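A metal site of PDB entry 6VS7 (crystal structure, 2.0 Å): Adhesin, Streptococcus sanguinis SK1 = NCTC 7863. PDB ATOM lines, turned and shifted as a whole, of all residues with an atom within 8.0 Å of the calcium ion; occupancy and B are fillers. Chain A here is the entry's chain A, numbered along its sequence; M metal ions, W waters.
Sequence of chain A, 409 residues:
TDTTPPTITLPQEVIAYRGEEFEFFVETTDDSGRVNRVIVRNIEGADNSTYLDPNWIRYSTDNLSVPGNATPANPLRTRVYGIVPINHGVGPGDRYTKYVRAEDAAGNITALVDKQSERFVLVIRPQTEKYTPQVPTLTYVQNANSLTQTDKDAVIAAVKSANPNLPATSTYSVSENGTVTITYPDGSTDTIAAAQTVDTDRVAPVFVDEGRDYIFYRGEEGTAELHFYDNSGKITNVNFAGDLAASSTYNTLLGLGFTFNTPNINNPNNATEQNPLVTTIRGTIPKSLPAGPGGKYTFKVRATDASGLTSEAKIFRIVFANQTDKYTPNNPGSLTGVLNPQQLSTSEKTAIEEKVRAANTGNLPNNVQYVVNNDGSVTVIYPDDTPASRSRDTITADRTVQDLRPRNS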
ATOM      1  N   PRO A 126      -3.444  -7.253  25.601  1.00  0.00           N
ATOM      2  CA  PRO A 126      -3.895  -8.554  26.090  1.00  0.00           C
ATOM      3  C   PRO A 126      -4.313  -9.459  24.946  1.00  0.00           C
ATOM      4  O   PRO A 126      -4.691  -9.016  23.863  1.00  0.00           O
ATOM      5  CB  PRO A 126      -5.089  -8.213  26.991  1.00  0.00           C
ATOM      6  CG  PRO A 126      -5.616  -6.924  26.430  1.00  0.00           C
ATOM      7  CD  PRO A 126      -4.360  -6.164  26.020  1.00  0.00           C
ATOM      8  N   GLN A 127      -4.266 -10.770  25.212  1.00  0.00           N
ATOM      9  CA  GLN A 127      -4.601 -11.721  24.159  1.00  0.00           C
ATOM     10  C   GLN A 127      -6.049 -11.577  23.689  1.00  0.00           C
ATOM     11  O   GLN A 127      -6.356 -11.921  22.549  1.00  0.00           O
ATOM     12  CB  GLN A 127      -4.343 -13.141  24.643  1.00  0.00           C
ATOM     13  CG  GLN A 127      -3.012 -13.696  24.203  1.00  0.00           C
ATOM     14  CD  GLN A 127      -2.817 -15.135  24.593  1.00  0.00           C
ATOM     15  OE1 GLN A 127      -3.105 -15.514  25.726  1.00  0.00           O
ATOM     16  NE2 GLN A 127      -2.313 -15.945  23.675  1.00  0.00           N
ATOM     17  N   THR A 128      -6.933 -11.072  24.542  1.00  0.00           N
ATOM     18  CA  THR A 128      -8.344 -10.920  24.151  1.00  0.00           C
ATOM     19  C   THR A 128      -8.528  -9.909  23.027  1.00  0.00           C
ATOM     20  O   THR A 128      -9.553  -9.949  22.342  1.00  0.00           O
ATOM     21  CB  THR A 128      -9.195 -10.525  25.363  1.00  0.00           C
ATOM     22  OG1 THR A 128     -10.563 -10.425  24.960  1.00  0.00           O
ATOM     23  CG2 THR A 128      -8.780  -9.175  25.901  1.00  0.00           C
ATOM     24  N   GLU A 129      -7.580  -8.985  22.828  1.00  0.00           N
ATOM     25  CA  GLU A 129      -7.741  -8.048  21.737  1.00  0.00           C
ATOM     26  C   GLU A 129      -7.419  -8.656  20.379  1.00  0.00           C
ATOM     27  O   GLU A 129      -7.862  -8.129  19.366  1.00  0.00           O
ATOM     28  CB  GLU A 129      -6.858  -6.821  21.960  1.00  0.00           C
ATOM     29  CG  GLU A 129      -7.399  -5.952  23.066  1.00  0.00           C
ATOM     30  CD  GLU A 129      -6.724  -4.591  23.130  1.00  0.00           C
ATOM     31  OE1 GLU A 129      -5.970  -4.226  22.192  1.00  0.00           O
ATOM     32  OE2 GLU A 129      -6.963  -3.900  24.136  1.00  0.00           O
ATOM     33  N   LYS A 130      -6.642  -9.736  20.353  1.00  0.00           N
ATOM     34  CA  LYS A 130      -6.354 -10.376  19.078  1.00  0.00           C
ATOM     35  C   LYS A 130      -7.510 -11.232  18.588  1.00  0.00           C
ATOM     36  O   LYS A 130      -7.739 -11.333  17.374  1.00  0.00           O
ATOM     37  CB  LYS A 130      -5.094 -11.248  19.207  1.00  0.00           C
ATOM     38  CG  LYS A 130      -4.729 -12.028  17.936  1.00  0.00           C
ATOM     39  CD  LYS A 130      -3.483 -12.850  18.185  1.00  0.00           C
ATOM     40  CE  LYS A 130      -2.999 -13.558  16.927  1.00  0.00           C
ATOM     41  NZ  LYS A 130      -1.899 -14.507  17.272  1.00  0.00           N
ATOM     42  N   TYR A 131      -8.273 -11.842  19.490  1.00  0.00           N
ATOM     43  CA  TYR A 131      -9.226 -12.886  19.130  1.00  0.00           C
ATOM     44  C   TYR A 131     -10.654 -12.370  19.261  1.00  0.00           C
ATOM     45  O   TYR A 131     -11.006 -11.752  20.269  1.00  0.00           O
ATOM     46  CB  TYR A 131      -9.010 -14.110  20.023  1.00  0.00           C
ATOM     47  CG  TYR A 131      -7.627 -14.693  19.876  1.00  0.00           C
ATOM     48  CD1 TYR A 131      -7.269 -15.433  18.752  1.00  0.00           C
ATOM     49  CD2 TYR A 131      -6.663 -14.492  20.854  1.00  0.00           C
ATOM     50  CE1 TYR A 131      -6.010 -15.961  18.617  1.00  0.00           C
ATOM     51  CE2 TYR A 131      -5.387 -15.021  20.717  1.00  0.00           C
ATOM     52  CZ  TYR A 131      -5.075 -15.765  19.602  1.00  0.00           C
ATOM     53  OH  TYR A 131      -3.810 -16.301  19.470  1.00  0.00           O
ATOM     54  N   THR A 132     -11.473 -12.633  18.247  1.00  0.00           N
ATOM     55  CA  THR A 132     -12.894 -12.334  18.316  1.00  0.00           C
ATOM     56  C   THR A 132     -13.667 -13.646  18.233  1.00  0.00           C
ATOM     57  O   THR A 132     -13.700 -14.270  17.156  1.00  0.00           O
ATOM     58  CB  THR A 132     -13.332 -11.402  17.183  1.00  0.00           C
ATOM     59  OG1 THR A 132     -12.362 -10.366  16.989  1.00  0.00           O
ATOM     60  CG2 THR A 132     -14.686 -10.764  17.545  1.00  0.00           C
ATOM     61  N   PRO A 133     -14.271 -14.113  19.322  1.00  0.00           N
ATOM     62  CA  PRO A 133     -14.927 -15.428  19.304  1.00  0.00           C
ATOM     63  C   PRO A 133     -16.163 -15.445  18.420  1.00  0.00           C
ATOM     64  O   PRO A 133     -16.928 -14.475  18.379  1.00  0.00           O
ATOM     65  CB  PRO A 133     -15.296 -15.668  20.777  1.00  0.00           C
ATOM     66  CG  PRO A 133     -14.385 -14.728  21.557  1.00  0.00           C
ATOM     67  CD  PRO A 133     -14.240 -13.528  20.672  1.00  0.00           C
ATOM     68  N   LEU A 166      -8.972 -19.962  18.010  1.00  0.00           N
ATOM     69  CA  LEU A 166      -8.572 -19.470  19.312  1.00  0.00           C
ATOM     70  C   LEU A 166      -7.386 -20.278  19.815  1.00  0.00           C
ATOM     71  O   LEU A 166      -7.178 -21.415  19.374  1.00  0.00           O
ATOM     72  CB  LEU A 166      -9.734 -19.548  20.296  1.00  0.00           C
ATOM     73  CG  LEU A 166     -10.958 -18.738  19.875  1.00  0.00           C
ATOM     74  CD1 LEU A 166     -12.053 -18.810  20.943  1.00  0.00           C
ATOM     75  CD2 LEU A 166     -10.586 -17.285  19.622  1.00  0.00           C
ATOM     76  N   TYR A 184      -8.079 -16.684  28.156  1.00  0.00           N
ATOM     77  CA  TYR A 184      -6.936 -16.874  27.267  1.00  0.00           C
ATOM     78  C   TYR A 184      -5.706 -17.249  28.075  1.00  0.00           C
ATOM     79  O   TYR A 184      -5.697 -17.116  29.293  1.00  0.00           O
ATOM     80  CB  TYR A 184      -6.714 -15.592  26.475  1.00  0.00           C
ATOM     81  CG  TYR A 184      -7.848 -15.347  25.520  1.00  0.00           C
ATOM     82  CD1 TYR A 184      -8.037 -16.175  24.428  1.00  0.00           C
ATOM     83  CD2 TYR A 184      -8.753 -14.316  25.736  1.00  0.00           C
ATOM     84  CE1 TYR A 184      -9.090 -15.981  23.552  1.00  0.00           C
ATOM     85  CE2 TYR A 184      -9.816 -14.116  24.866  1.00  0.00           C
ATOM     86  CZ  TYR A 184      -9.977 -14.952  23.767  1.00  0.00           C
ATOM     87  OH  TYR A 184     -11.008 -14.759  22.880  1.00  0.00           O
ATOM     88  N   SER A 188      -6.395 -12.945  30.271  1.00  0.00           N
ATOM     89  CA  SER A 188      -7.430 -12.054  29.788  1.00  0.00           C
ATOM     90  C   SER A 188      -8.622 -12.878  29.278  1.00  0.00           C
ATOM     91  O   SER A 188      -8.525 -14.072  29.013  1.00  0.00           O
ATOM     92  CB  SER A 188      -6.876 -11.124  28.699  1.00  0.00           C
ATOM     93  OG  SER A 188      -6.384 -11.841  27.571  1.00  0.00           O
ATOM     94  N   THR A 189      -9.776 -12.235  29.201  1.00  0.00           N
ATOM     95  CA  THR A 189     -10.997 -12.999  28.999  1.00  0.00           C
ATOM     96  C   THR A 189     -11.838 -12.410  27.878  1.00  0.00           C
ATOM     97  O   THR A 189     -11.629 -11.284  27.418  1.00  0.00           O
ATOM     98  CB  THR A 189     -11.857 -13.089  30.268  1.00  0.00           C
ATOM     99  OG1 THR A 189     -12.533 -11.849  30.472  1.00  0.00           O
ATOM    100  CG2 THR A 189     -11.018 -13.415  31.489  1.00  0.00           C
ATOM    101  N   ASP A 190     -12.830 -13.209  27.482  1.00  0.00           N
ATOM    102  CA  ASP A 190     -13.900 -12.800  26.582  1.00  0.00           C
ATOM    103  C   ASP A 190     -15.168 -13.504  27.022  1.00  0.00           C
ATOM    104  O   ASP A 190     -15.120 -14.543  27.677  1.00  0.00           O
ATOM    105  CB  ASP A 190     -13.580 -13.127  25.141  1.00  0.00           C
ATOM    106  CG  ASP A 190     -13.657 -11.930  24.245  1.00  0.00           C
ATOM    107  OD1 ASP A 190     -14.432 -11.005  24.577  1.00  0.00           O
ATOM    108  OD2 ASP A 190     -12.950 -11.926  23.220  1.00  0.00           O
ATOM    109  N   THR A 191     -16.311 -12.948  26.638  1.00  0.00           N
ATOM    110  CA  THR A 191     -17.608 -13.480  27.068  1.00  0.00           C
ATOM    111  C   THR A 191     -18.513 -13.685  25.870  1.00  0.00           C
ATOM    112  O   THR A 191     -18.564 -12.837  24.976  1.00  0.00           O
ATOM    113  CB  THR A 191     -18.277 -12.549  28.081  1.00  0.00           C
ATOM    114  OG1 THR A 191     -17.478 -12.473  29.260  1.00  0.00           O
ATOM    115  CG2 THR A 191     -19.641 -13.068  28.474  1.00  0.00           C
HETATM  116 CA    CA M   1     -11.802 -10.266  22.357  1.00  0.00          CA
HETATM  117  O   HOH W   1     -11.920  -8.824  20.125  1.00  0.00           O
HETATM  118  O   HOH W   2     -12.274  -8.464  24.019  1.00  0.00           O
HETATM  119  O   HOH W   3     -14.421 -10.057  21.216  1.00  0.00           O
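The side-chain amino group of Lys 130 sits at hydrogen-bond distance from the side-chain hydroxyl of Tyr 131, 3.4 Å away. The side-chain hydroxyl (OG) of Ser 188 sits at hydrogen-bond distance from the backbone NH (N) of Thr 128 (3.2 Å). The side-chain carboxylate of Asp 190 lies close to the side-chain hydroxyl of Tyr 184 (3.5 Å). The side-chain hydroxyl of Thr 128 sits close to the backbone carbonyl oxygen of Thr 189 (2.8 Å).
The calcium ion is bound by OD2 of Asp 190, at 2.2 Å. The calcium ion is bound by the backbone carbonyl oxygen (O) of Thr 128, 2.3 Å away. Water W2 binds the calcium ion (2.5 Å). Water W1 binds the calcium ion (2.7 Å). O of Tyr 131 binds the calcium ion. Water W3 binds the calcium ion (2.9 Å). The calcium ion is bound by OG1 of Thr 128 (2.9 Å). The calcium ion has seven donor atoms within binding distance.
Within 4 Å of the calcium ion: Thr 128, Tyr 131 and Asp 190. The nearest printed residue that does not touch the calcium ion is Pro 133 (4.4 Å).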
